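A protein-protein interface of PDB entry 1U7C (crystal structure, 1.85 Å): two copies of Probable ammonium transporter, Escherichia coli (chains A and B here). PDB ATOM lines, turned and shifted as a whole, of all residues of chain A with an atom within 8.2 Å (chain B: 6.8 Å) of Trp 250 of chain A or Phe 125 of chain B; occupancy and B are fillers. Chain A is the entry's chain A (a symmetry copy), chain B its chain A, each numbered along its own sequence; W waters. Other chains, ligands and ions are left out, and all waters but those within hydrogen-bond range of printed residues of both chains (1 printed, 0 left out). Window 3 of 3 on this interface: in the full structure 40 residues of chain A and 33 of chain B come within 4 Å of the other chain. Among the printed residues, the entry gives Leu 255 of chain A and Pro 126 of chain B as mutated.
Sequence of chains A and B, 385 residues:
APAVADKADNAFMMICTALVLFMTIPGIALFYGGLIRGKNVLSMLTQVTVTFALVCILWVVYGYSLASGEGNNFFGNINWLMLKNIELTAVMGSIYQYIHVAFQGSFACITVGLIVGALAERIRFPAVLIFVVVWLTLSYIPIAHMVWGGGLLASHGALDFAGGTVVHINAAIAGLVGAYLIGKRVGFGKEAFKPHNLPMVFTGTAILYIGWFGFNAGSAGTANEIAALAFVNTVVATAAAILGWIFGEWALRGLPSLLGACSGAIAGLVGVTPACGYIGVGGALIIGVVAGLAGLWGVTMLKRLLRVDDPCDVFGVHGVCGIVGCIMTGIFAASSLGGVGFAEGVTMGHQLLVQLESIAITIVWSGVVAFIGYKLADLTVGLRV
Among the printed residues, merely in contact across the chains: Leu 243 of chain A with Val 50 of chain B (3.8 Å), Ile 246 of chain A with Val 50 of chain B (3.6 Å), Trp 250 of chain A with Phe 125 of chain B (2.9 Å), Trp 250 of chain A with Leu 129 of chain B (3.7 Å), Pro 256 of chain A with Phe 125 of chain B (3.6 Å) and Ser 257 of chain A with Thr 46 of chain B (3.7 Å).
OG of Ser 257 of chain A sits at hydrogen-bond distance from OE2 of Glu 249 of chain A (2.5 Å). O of Gly 254 of chain A lies close to NE1 of Trp 250 of chain A (3.3 Å).
Water W1 bridges O of Pro 256 of chain A (3.1 Å) and OG1 of Thr 46 of chain B (3.4 Å).
Among the printed residues, 7 pairs touch across the chains. Among the printed residues, no Asp or Glu carboxylate lies within 4 Å of a Lys or Arg side-chain nitrogen of the other chain.
Gly 244 of chain A touches none of the printed residues of chain B. Of the printed residues of chain B, Ile 246 of chain A touches Val 50. Ser 43 of chain B touches none of the printed residues of chain A. Phe 125 of chain B touches just these residues of chain A: Trp 250 and Pro 256. Of the printed residues of chain A, Leu 129 of chain B touches Trp 250 (3.7 Å). The nearest residue of chain B that does not touch Trp 250 of chain A is Pro 126 of chain B (4.1 Å).
No position is printed for both chains.
The backbone NH of Leu 258 of chain A sits at hydrogen-bond distance from the side-chain hydroxyl of Thr 46 of chain B, 3.1 Å away.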
ATOM      1  N   ILE A 242      14.492 -10.692  -3.764  1.00  0.00           N
ATOM      2  CA  ILE A 242      15.835 -11.089  -4.144  1.00  0.00           C
ATOM      3  C   ILE A 242      16.608 -11.294  -2.849  1.00  0.00           C
ATOM      4  O   ILE A 242      17.284 -12.302  -2.670  1.00  0.00           O
ATOM      5  CB  ILE A 242      16.533 -10.001  -4.987  1.00  0.00           C
ATOM      6  CG1 ILE A 242      15.941  -9.979  -6.400  1.00  0.00           C
ATOM      7  CG2 ILE A 242      18.037 -10.260  -5.034  1.00  0.00           C
ATOM      8  CD1 ILE A 242      16.348  -8.758  -7.213  1.00  0.00           C
ATOM      9  N   LEU A 243      16.478 -10.339  -1.935  1.00  0.00           N
ATOM     10  CA  LEU A 243      17.178 -10.425  -0.664  1.00  0.00           C
ATOM     11  C   LEU A 243      16.639 -11.558   0.192  1.00  0.00           C
ATOM     12  O   LEU A 243      17.407 -12.273   0.836  1.00  0.00           O
ATOM     13  CB  LEU A 243      17.075  -9.094   0.079  1.00  0.00           C
ATOM     14  CG  LEU A 243      17.710  -7.915  -0.665  1.00  0.00           C
ATOM     15  CD1 LEU A 243      17.515  -6.643   0.143  1.00  0.00           C
ATOM     16  CD2 LEU A 243      19.195  -8.177  -0.897  1.00  0.00           C
ATOM     17  N   GLY A 244      15.319 -11.727   0.196  1.00  0.00           N
ATOM     18  CA  GLY A 244      14.728 -12.797   0.978  1.00  0.00           C
ATOM     19  C   GLY A 244      15.205 -14.154   0.498  1.00  0.00           C
ATOM     20  O   GLY A 244      15.627 -14.989   1.298  1.00  0.00           O
ATOM     21  N   TRP A 245      15.154 -14.378  -0.811  1.00  0.00           N
ATOM     22  CA  TRP A 245      15.587 -15.648  -1.377  1.00  0.00           C
ATOM     23  C   TRP A 245      17.068 -15.880  -1.103  1.00  0.00           C
ATOM     24  O   TRP A 245      17.459 -16.937  -0.613  1.00  0.00           O
ATOM     25  CB  TRP A 245      15.337 -15.675  -2.890  1.00  0.00           C
ATOM     26  CG  TRP A 245      15.560 -17.024  -3.514  1.00  0.00           C
ATOM     27  CD1 TRP A 245      16.711 -17.766  -3.496  1.00  0.00           C
ATOM     28  CD2 TRP A 245      14.599 -17.795  -4.243  1.00  0.00           C
ATOM     29  NE1 TRP A 245      16.522 -18.947  -4.165  1.00  0.00           N
ATOM     30  CE2 TRP A 245      15.236 -18.994  -4.635  1.00  0.00           C
ATOM     31  CE3 TRP A 245      13.261 -17.591  -4.603  1.00  0.00           C
ATOM     32  CZ2 TRP A 245      14.579 -19.987  -5.373  1.00  0.00           C
ATOM     33  CZ3 TRP A 245      12.607 -18.578  -5.339  1.00  0.00           C
ATOM     34  CH2 TRP A 245      13.270 -19.763  -5.713  1.00  0.00           C
ATOM     35  N   ILE A 246      17.889 -14.887  -1.433  1.00  0.00           N
ATOM     36  CA  ILE A 246      19.330 -14.980  -1.233  1.00  0.00           C
ATOM     37  C   ILE A 246      19.687 -15.213   0.230  1.00  0.00           C
ATOM     38  O   ILE A 246      20.631 -15.944   0.536  1.00  0.00           O
ATOM     39  CB  ILE A 246      20.037 -13.703  -1.755  1.00  0.00           C
ATOM     40  CG1 ILE A 246      20.081 -13.735  -3.286  1.00  0.00           C
ATOM     41  CG2 ILE A 246      21.444 -13.587  -1.177  1.00  0.00           C
ATOM     42  CD1 ILE A 246      20.933 -14.853  -3.853  1.00  0.00           C
ATOM     43  N   PHE A 247      18.938 -14.592   1.134  1.00  0.00           N
ATOM     44  CA  PHE A 247      19.190 -14.764   2.558  1.00  0.00           C
ATOM     45  C   PHE A 247      18.882 -16.208   2.933  1.00  0.00           C
ATOM     46  O   PHE A 247      19.680 -16.871   3.595  1.00  0.00           O
ATOM     47  CB  PHE A 247      18.304 -13.830   3.379  1.00  0.00           C
ATOM     48  CG  PHE A 247      18.485 -13.983   4.861  1.00  0.00           C
ATOM     49  CD1 PHE A 247      19.618 -13.481   5.493  1.00  0.00           C
ATOM     50  CD2 PHE A 247      17.537 -14.661   5.621  1.00  0.00           C
ATOM     51  CE1 PHE A 247      19.808 -13.655   6.861  1.00  0.00           C
ATOM     52  CE2 PHE A 247      17.716 -14.840   6.992  1.00  0.00           C
ATOM     53  CZ  PHE A 247      18.855 -14.336   7.612  1.00  0.00           C
ATOM     54  N   GLY A 248      17.721 -16.686   2.501  1.00  0.00           N
ATOM     55  CA  GLY A 248      17.329 -18.053   2.799  1.00  0.00           C
ATOM     56  C   GLY A 248      18.292 -19.051   2.188  1.00  0.00           C
ATOM     57  O   GLY A 248      18.668 -20.043   2.813  1.00  0.00           O
ATOM     58  N   GLU A 249      18.696 -18.788   0.953  1.00  0.00           N
ATOM     59  CA  GLU A 249      19.618 -19.665   0.257  1.00  0.00           C
ATOM     60  C   GLU A 249      20.956 -19.691   0.976  1.00  0.00           C
ATOM     61  O   GLU A 249      21.580 -20.741   1.130  1.00  0.00           O
ATOM     62  CB  GLU A 249      19.807 -19.175  -1.177  1.00  0.00           C
ATOM     63  CG  GLU A 249      20.853 -19.926  -1.959  1.00  0.00           C
ATOM     64  CD  GLU A 249      20.910 -19.476  -3.401  1.00  0.00           C
ATOM     65  OE1 GLU A 249      20.956 -18.250  -3.635  1.00  0.00           O
ATOM     66  OE2 GLU A 249      20.913 -20.346  -4.293  1.00  0.00           O
ATOM     67  N   TRP A 250      21.384 -18.520   1.426  1.00  0.00           N
ATOM     68  CA  TRP A 250      22.646 -18.385   2.129  1.00  0.00           C
ATOM     69  C   TRP A 250      22.641 -19.181   3.426  1.00  0.00           C
ATOM     70  O   TRP A 250      23.630 -19.819   3.781  1.00  0.00           O
ATOM     71  CB  TRP A 250      22.885 -16.922   2.452  1.00  0.00           C
ATOM     72  CG  TRP A 250      24.272 -16.478   2.245  1.00  0.00           C
ATOM     73  CD1 TRP A 250      25.408 -17.223   2.385  1.00  0.00           C
ATOM     74  CD2 TRP A 250      24.690 -15.152   1.954  1.00  0.00           C
ATOM     75  NE1 TRP A 250      26.514 -16.431   2.201  1.00  0.00           N
ATOM     76  CE2 TRP A 250      26.100 -15.150   1.934  1.00  0.00           C
ATOM     77  CE3 TRP A 250      24.007 -13.953   1.709  1.00  0.00           C
ATOM     78  CZ2 TRP A 250      26.842 -13.996   1.684  1.00  0.00           C
ATOM     79  CZ3 TRP A 250      24.740 -12.809   1.463  1.00  0.00           C
ATOM     80  CH2 TRP A 250      26.144 -12.840   1.454  1.00  0.00           C
ATOM     81  N   ALA A 251      21.519 -19.132   4.132  1.00  0.00           N
ATOM     82  CA  ALA A 251      21.381 -19.836   5.397  1.00  0.00           C
ATOM     83  C   ALA A 251      21.125 -21.321   5.184  1.00  0.00           C
ATOM     84  O   ALA A 251      21.365 -22.135   6.075  1.00  0.00           O
ATOM     85  CB  ALA A 251      20.249 -19.223   6.209  1.00  0.00           C
ATOM     86  N   LEU A 252      20.646 -21.671   3.995  1.00  0.00           N
ATOM     87  CA  LEU A 252      20.345 -23.059   3.669  1.00  0.00           C
ATOM     88  C   LEU A 252      21.502 -23.763   2.965  1.00  0.00           C
ATOM     89  O   LEU A 252      21.747 -24.949   3.194  1.00  0.00           O
ATOM     90  CB  LEU A 252      19.104 -23.127   2.776  1.00  0.00           C
ATOM     91  CG  LEU A 252      18.618 -24.517   2.360  1.00  0.00           C
ATOM     92  CD1 LEU A 252      17.916 -25.189   3.533  1.00  0.00           C
ATOM     93  CD2 LEU A 252      17.667 -24.390   1.179  1.00  0.00           C
ATOM     94  N   ARG A 253      22.213 -23.030   2.115  1.00  0.00           N
ATOM     95  CA  ARG A 253      23.320 -23.603   1.360  1.00  0.00           C
ATOM     96  C   ARG A 253      24.686 -23.005   1.691  1.00  0.00           C
ATOM     97  O   ARG A 253      25.709 -23.469   1.190  1.00  0.00           O
ATOM     98  CB  ARG A 253      23.036 -23.460  -0.137  1.00  0.00           C
ATOM     99  CG  ARG A 253      21.717 -24.091  -0.555  1.00  0.00           C
ATOM    100  CD  ARG A 253      21.729 -25.592  -0.300  1.00  0.00           C
ATOM    101  NE  ARG A 253      20.389 -26.171  -0.267  1.00  0.00           N
ATOM    102  CZ  ARG A 253      19.523 -26.128  -1.273  1.00  0.00           C
ATOM    103  NH1 ARG A 253      19.846 -25.527  -2.409  1.00  0.00           N
ATOM    104  NH2 ARG A 253      18.327 -26.690  -1.143  1.00  0.00           N
ATOM    105  N   GLY A 254      24.703 -21.975   2.531  1.00  0.00           N
ATOM    106  CA  GLY A 254      25.961 -21.359   2.910  1.00  0.00           C
ATOM    107  C   GLY A 254      26.471 -20.308   1.941  1.00  0.00           C
ATOM    108  O   GLY A 254      27.466 -19.637   2.213  1.00  0.00           O
ATOM    109  N   LEU A 255      25.797 -20.161   0.807  1.00  0.00           N
ATOM    110  CA  LEU A 255      26.206 -19.175  -0.180  1.00  0.00           C
ATOM    111  C   LEU A 255      25.093 -18.805  -1.145  1.00  0.00           C
ATOM    112  O   LEU A 255      24.233 -19.621  -1.463  1.00  0.00           O
ATOM    113  CB  LEU A 255      27.418 -19.676  -0.974  1.00  0.00           C
ATOM    114  CG  LEU A 255      27.471 -21.122  -1.489  1.00  0.00           C
ATOM    115  CD1 LEU A 255      26.149 -21.549  -2.100  1.00  0.00           C
ATOM    116  CD2 LEU A 255      28.591 -21.228  -2.512  1.00  0.00           C
ATOM    117  N   PRO A 256      25.087 -17.551  -1.614  1.00  0.00           N
ATOM    118  CA  PRO A 256      24.054 -17.124  -2.555  1.00  0.00           C
ATOM    119  C   PRO A 256      24.432 -17.648  -3.934  1.00  0.00           C
ATOM    120  O   PRO A 256      25.578 -18.032  -4.160  1.00  0.00           O
ATOM    121  CB  PRO A 256      24.136 -15.605  -2.474  1.00  0.00           C
ATOM    122  CG  PRO A 256      25.606 -15.379  -2.281  1.00  0.00           C
ATOM    123  CD  PRO A 256      25.967 -16.428  -1.248  1.00  0.00           C
ATOM    124  N   SER A 257      23.472 -17.690  -4.849  1.00  0.00           N
ATOM    125  CA  SER A 257      23.756 -18.151  -6.199  1.00  0.00           C
ATOM    126  C   SER A 257      23.025 -17.240  -7.168  1.00  0.00           C
ATOM    127  O   SER A 257      22.042 -16.595  -6.796  1.00  0.00           O
ATOM    128  CB  SER A 257      23.281 -19.589  -6.403  1.00  0.00           C
ATOM    129  OG  SER A 257      21.868 -19.658  -6.473  1.00  0.00           O
ATOM    130  N   LEU A 258      23.503 -17.190  -8.404  1.00  0.00           N
ATOM    131  CA  LEU A 258      22.878 -16.349  -9.413  1.00  0.00           C
ATOM    132  C   LEU A 258      21.441 -16.792  -9.633  1.00  0.00           C
ATOM    133  O   LEU A 258      20.533 -15.971  -9.693  1.00  0.00           O
ATOM    134  CB  LEU A 258      23.650 -16.427 -10.730  1.00  0.00           C
ATOM    135  CG  LEU A 258      23.034 -15.616 -11.873  1.00  0.00           C
ATOM    136  CD1 LEU A 258      22.899 -14.155 -11.456  1.00  0.00           C
ATOM    137  CD2 LEU A 258      23.894 -15.750 -13.119  1.00  0.00           C
ATOM    138  N   ALA A 261      19.319 -15.555  -6.897  1.00  0.00           N
ATOM    139  CA  ALA A 261      19.034 -14.132  -7.013  1.00  0.00           C
ATOM    140  C   ALA A 261      17.956 -13.890  -8.058  1.00  0.00           C
ATOM    141  O   ALA A 261      17.037 -13.106  -7.840  1.00  0.00           O
ATOM    142  CB  ALA A 261      20.303 -13.372  -7.376  1.00  0.00           C
ATOM    143  N   LEU A 296      11.629 -19.962  -2.522  1.00  0.00           N
ATOM    144  CA  LEU A 296      12.751 -20.840  -2.211  1.00  0.00           C
ATOM    145  C   LEU A 296      12.206 -22.143  -1.636  1.00  0.00           C
ATOM    146  O   LEU A 296      12.645 -23.231  -2.006  1.00  0.00           O
ATOM    147  CB  LEU A 296      13.680 -20.170  -1.198  1.00  0.00           C
ATOM    148  CG  LEU A 296      14.826 -21.030  -0.655  1.00  0.00           C
ATOM    149  CD1 LEU A 296      15.695 -21.543  -1.798  1.00  0.00           C
ATOM    150  CD2 LEU A 296      15.652 -20.200   0.315  1.00  0.00           C
ATOM    151  N   SER B  43      29.356 -14.971 -10.352  1.00  0.00           N
ATOM    152  CA  SER B  43      29.512 -14.248  -9.096  1.00  0.00           C
ATOM    153  C   SER B  43      29.202 -12.770  -9.285  1.00  0.00           C
ATOM    154  O   SER B  43      28.528 -12.154  -8.466  1.00  0.00           O
ATOM    155  CB  SER B  43      30.940 -14.406  -8.564  1.00  0.00           C
ATOM    156  OG  SER B  43      31.249 -15.764  -8.317  1.00  0.00           O
ATOM    157  N   THR B  46      25.524 -12.213  -9.705  1.00  0.00           N
ATOM    158  CA  THR B  46      24.846 -12.381  -8.430  1.00  0.00           C
ATOM    159  C   THR B  46      25.044 -11.123  -7.597  1.00  0.00           C
ATOM    160  O   THR B  46      24.099 -10.595  -7.014  1.00  0.00           O
ATOM    161  CB  THR B  46      25.394 -13.600  -7.658  1.00  0.00           C
ATOM    162  OG1 THR B  46      25.358 -14.755  -8.504  1.00  0.00           O
ATOM    163  CG2 THR B  46      24.551 -13.868  -6.419  1.00  0.00           C
ATOM    164  N   GLN B  47      26.277 -10.632  -7.547  1.00  0.00           N
ATOM    165  CA  GLN B  47      26.548  -9.432  -6.774  1.00  0.00           C
ATOM    166  C   GLN B  47      25.813  -8.218  -7.315  1.00  0.00           C
ATOM    167  O   GLN B  47      25.269  -7.428  -6.546  1.00  0.00           O
ATOM    168  CB  GLN B  47      28.045  -9.157  -6.720  1.00  0.00           C
ATOM    169  CG  GLN B  47      28.755 -10.026  -5.706  1.00  0.00           C
ATOM    170  CD  GLN B  47      30.156  -9.543  -5.426  1.00  0.00           C
ATOM    171  OE1 GLN B  47      30.444  -8.355  -5.545  1.00  0.00           O
ATOM    172  NE2 GLN B  47      31.031 -10.457  -5.031  1.00  0.00           N
ATOM    173  N   VAL B  48      25.786  -8.065  -8.633  1.00  0.00           N
ATOM    174  CA  VAL B  48      25.090  -6.930  -9.212  1.00  0.00           C
ATOM    175  C   VAL B  48      23.604  -7.010  -8.881  1.00  0.00           C
ATOM    176  O   VAL B  48      22.986  -6.014  -8.515  1.00  0.00           O
ATOM    177  CB  VAL B  48      25.272  -6.883 -10.743  1.00  0.00           C
ATOM    178  CG1 VAL B  48      24.337  -5.856 -11.357  1.00  0.00           C
ATOM    179  CG2 VAL B  48      26.712  -6.520 -11.074  1.00  0.00           C
ATOM    180  N   VAL B  50      22.051  -8.737  -6.367  1.00  0.00           N
ATOM    181  CA  VAL B  50      21.770  -8.583  -4.949  1.00  0.00           C
ATOM    182  C   VAL B  50      22.029  -7.162  -4.461  1.00  0.00           C
ATOM    183  O   VAL B  50      21.249  -6.635  -3.674  1.00  0.00           O
ATOM    184  CB  VAL B  50      22.577  -9.588  -4.112  1.00  0.00           C
ATOM    185  CG1 VAL B  50      22.357  -9.331  -2.629  1.00  0.00           C
ATOM    186  CG2 VAL B  50      22.145 -11.005  -4.467  1.00  0.00           C
ATOM    187  N   THR B  51      23.113  -6.536  -4.913  1.00  0.00           N
ATOM    188  CA  THR B  51      23.374  -5.168  -4.479  1.00  0.00           C
ATOM    189  C   THR B  51      22.324  -4.227  -5.068  1.00  0.00           C
ATOM    190  O   THR B  51      21.984  -3.213  -4.464  1.00  0.00           O
ATOM    191  CB  THR B  51      24.801  -4.689  -4.855  1.00  0.00           C
ATOM    192  OG1 THR B  51      25.036  -4.865  -6.257  1.00  0.00           O
ATOM    193  CG2 THR B  51      25.832  -5.479  -4.063  1.00  0.00           C
ATOM    194  N   ALA B 120      33.063  -6.799  -8.396  1.00  0.00           N
ATOM    195  CA  ALA B 120      32.476  -8.019  -7.850  1.00  0.00           C
ATOM    196  C   ALA B 120      33.398  -9.232  -7.875  1.00  0.00           C
ATOM    197  O   ALA B 120      33.510  -9.960  -6.887  1.00  0.00           O
ATOM    198  CB  ALA B 120      31.183  -8.344  -8.590  1.00  0.00           C
ATOM    199  N   ILE B 123      35.950  -9.021  -4.990  1.00  0.00           N
ATOM    200  CA  ILE B 123      35.504  -8.703  -3.642  1.00  0.00           C
ATOM    201  C   ILE B 123      34.564  -9.766  -3.076  1.00  0.00           C
ATOM    202  O   ILE B 123      33.708 -10.297  -3.785  1.00  0.00           O
ATOM    203  CB  ILE B 123      34.798  -7.322  -3.608  1.00  0.00           C
ATOM    204  CG1 ILE B 123      34.432  -6.955  -2.171  1.00  0.00           C
ATOM    205  CG2 ILE B 123      33.551  -7.351  -4.484  1.00  0.00           C
ATOM    206  CD1 ILE B 123      33.951  -5.526  -2.010  1.00  0.00           C
ATOM    207  N   ARG B 124      34.744 -10.089  -1.801  1.00  0.00           N
ATOM    208  CA  ARG B 124      33.898 -11.077  -1.142  1.00  0.00           C
ATOM    209  C   ARG B 124      32.460 -10.580  -1.175  1.00  0.00           C
ATOM    210  O   ARG B 124      32.208  -9.382  -1.047  1.00  0.00           O
ATOM    211  CB  ARG B 124      34.338 -11.278   0.309  1.00  0.00           C
ATOM    212  CG  ARG B 124      35.671 -11.987   0.464  1.00  0.00           C
ATOM    213  CD  ARG B 124      36.010 -12.168   1.935  1.00  0.00           C
ATOM    214  NE  ARG B 124      34.911 -12.790   2.666  1.00  0.00           N
ATOM    215  CZ  ARG B 124      34.451 -14.013   2.429  1.00  0.00           C
ATOM    216  NH1 ARG B 124      34.996 -14.758   1.475  1.00  0.00           N
ATOM    217  NH2 ARG B 124      33.441 -14.493   3.142  1.00  0.00           N
ATOM    218  N   PHE B 125      31.518 -11.499  -1.341  1.00  0.00           N
ATOM    219  CA  PHE B 125      30.113 -11.122  -1.407  1.00  0.00           C
ATOM    220  C   PHE B 125      29.666 -10.322  -0.182  1.00  0.00           C
ATOM    221  O   PHE B 125      29.089  -9.249  -0.319  1.00  0.00           O
ATOM    222  CB  PHE B 125      29.248 -12.374  -1.588  1.00  0.00           C
ATOM    223  CG  PHE B 125      27.825 -12.078  -1.971  1.00  0.00           C
ATOM    224  CD1 PHE B 125      26.935 -11.571  -1.032  1.00  0.00           C
ATOM    225  CD2 PHE B 125      27.374 -12.304  -3.270  1.00  0.00           C
ATOM    226  CE1 PHE B 125      25.617 -11.293  -1.370  1.00  0.00           C
ATOM    227  CE2 PHE B 125      26.054 -12.029  -3.626  1.00  0.00           C
ATOM    228  CZ  PHE B 125      25.175 -11.522  -2.671  1.00  0.00           C
ATOM    229  N   PRO B 126      29.910 -10.765   1.093  1.00  0.00           N
ATOM    230  CA  PRO B 126      29.544 -10.118   2.230  1.00  0.00           C
ATOM    231  C   PRO B 126      30.189  -8.691   2.299  1.00  0.00           C
ATOM    232  O   PRO B 126      29.619  -7.716   2.806  1.00  0.00           O
ATOM    233  CB  PRO B 126      30.039 -10.880   3.465  1.00  0.00           C
ATOM    234  CG  PRO B 126      30.913 -11.384   2.658  1.00  0.00           C
ATOM    235  CD  PRO B 126      30.538 -12.209   1.502  1.00  0.00           C
ATOM    236  N   ALA B 127      31.404  -8.629   1.769  1.00  0.00           N
ATOM    237  CA  ALA B 127      32.129  -7.366   1.753  1.00  0.00           C
ATOM    238  C   ALA B 127      31.503  -6.338   0.814  1.00  0.00           C
ATOM    239  O   ALA B 127      31.481  -5.148   1.124  1.00  0.00           O
ATOM    240  CB  ALA B 127      33.579  -7.605   1.365  1.00  0.00           C
ATOM    241  N   VAL B 128      31.002  -6.789  -0.330  1.00  0.00           N
ATOM    242  CA  VAL B 128      30.401  -5.855  -1.273  1.00  0.00           C
ATOM    243  C   VAL B 128      29.114  -5.290  -0.685  1.00  0.00           C
ATOM    244  O   VAL B 128      28.776  -4.130  -0.912  1.00  0.00           O
ATOM    245  CB  VAL B 128      30.118  -6.523  -2.647  1.00  0.00           C
ATOM    246  CG1 VAL B 128      28.877  -7.394  -2.579  1.00  0.00           C
ATOM    247  CG2 VAL B 128      29.973  -5.454  -3.717  1.00  0.00           C
ATOM    248  N   LEU B 129      28.402  -6.110   0.083  1.00  0.00           N
ATOM    249  CA  LEU B 129      27.163  -5.669   0.708  1.00  0.00           C
ATOM    250  C   LEU B 129      27.476  -4.572   1.716  1.00  0.00           C
ATOM    251  O   LEU B 129      26.808  -3.540   1.758  1.00  0.00           O
ATOM    252  CB  LEU B 129      26.473  -6.845   1.406  1.00  0.00           C
ATOM    253  CG  LEU B 129      26.042  -7.988   0.481  1.00  0.00           C
ATOM    254  CD1 LEU B 129      25.499  -9.143   1.307  1.00  0.00           C
ATOM    255  CD2 LEU B 129      24.991  -7.481  -0.497  1.00  0.00           C
ATOM    256  N   ILE B 130      28.505  -4.798   2.524  1.00  0.00           N
ATOM    257  CA  ILE B 130      28.904  -3.812   3.515  1.00  0.00           C
ATOM    258  C   ILE B 130      29.348  -2.536   2.810  1.00  0.00           C
ATOM    259  O   ILE B 130      28.963  -1.437   3.202  1.00  0.00           O
ATOM    260  CB  ILE B 130      30.054  -4.352   4.394  1.00  0.00           C
ATOM    261  CG1 ILE B 130      29.528  -5.498   5.265  1.00  0.00           C
ATOM    262  CG2 ILE B 130      30.636  -3.234   5.249  1.00  0.00           C
ATOM    263  CD1 ILE B 130      30.602  -6.242   6.026  1.00  0.00           C
ATOM    264  N   VAL B 381      34.700  -8.461   7.469  1.00  0.00           N
ATOM    265  CA  VAL B 381      34.574  -9.762   6.821  1.00  0.00           C
ATOM    266  C   VAL B 381      35.708 -10.113   5.867  1.00  0.00           C
ATOM    267  O   VAL B 381      35.852 -11.267   5.463  1.00  0.00           O
ATOM    268  CB  VAL B 381      33.251  -9.840   6.032  1.00  0.00           C
ATOM    269  CG1 VAL B 381      32.074  -9.630   6.968  1.00  0.00           C
ATOM    270  CG2 VAL B 381      33.242  -8.789   4.927  1.00  0.00           C
ATOM    271  N   GLY B 382      36.516  -9.122   5.513  1.00  0.00           N
ATOM    272  CA  GLY B 382      37.603  -9.362   4.585  1.00  0.00           C
ATOM    273  C   GLY B 382      37.157  -8.963   3.192  1.00  0.00           C
ATOM    274  O   GLY B 382      36.113  -9.412   2.716  1.00  0.00           O
ATOM    275  N   LEU B 383      37.941  -8.111   2.544  1.00  0.00           N
ATOM    276  CA  LEU B 383      37.633  -7.623   1.202  1.00  0.00           C
ATOM    277  C   LEU B 383      37.915  -8.610   0.081  1.00  0.00           C
ATOM    278  O   LEU B 383      37.007  -9.084  -0.604  1.00  0.00           O
ATOM    279  CB  LEU B 383      38.434  -6.352   0.911  1.00  0.00           C
ATOM    280  CG  LEU B 383      37.872  -4.969   1.223  1.00  0.00           C
ATOM    281  CD1 LEU B 383      38.978  -3.937   1.049  1.00  0.00           C
ATOM    282  CD2 LEU B 383      36.702  -4.665   0.294  1.00  0.00           C
ATOM    283  N   VAL B 385      38.835 -11.683  -2.369  1.00  0.00           N
ATOM    284  CA  VAL B 385      38.353 -13.039  -2.585  1.00  0.00           C
ATOM    285  C   VAL B 385      39.504 -14.020  -2.413  1.00  0.00           C
ATOM    286  O   VAL B 385      40.575 -13.777  -3.007  1.00  0.00           O
ATOM    287  CB  VAL B 385      37.770 -13.188  -4.011  1.00  0.00           C
ATOM    288  CG1 VAL B 385      37.906 -14.625  -4.493  1.00  0.00           C
ATOM    289  CG2 VAL B 385      36.311 -12.771  -4.015  1.00  0.00           C
HETATM  290  O   HOH W   1      27.134 -16.925  -6.611  1.00  0.00           O
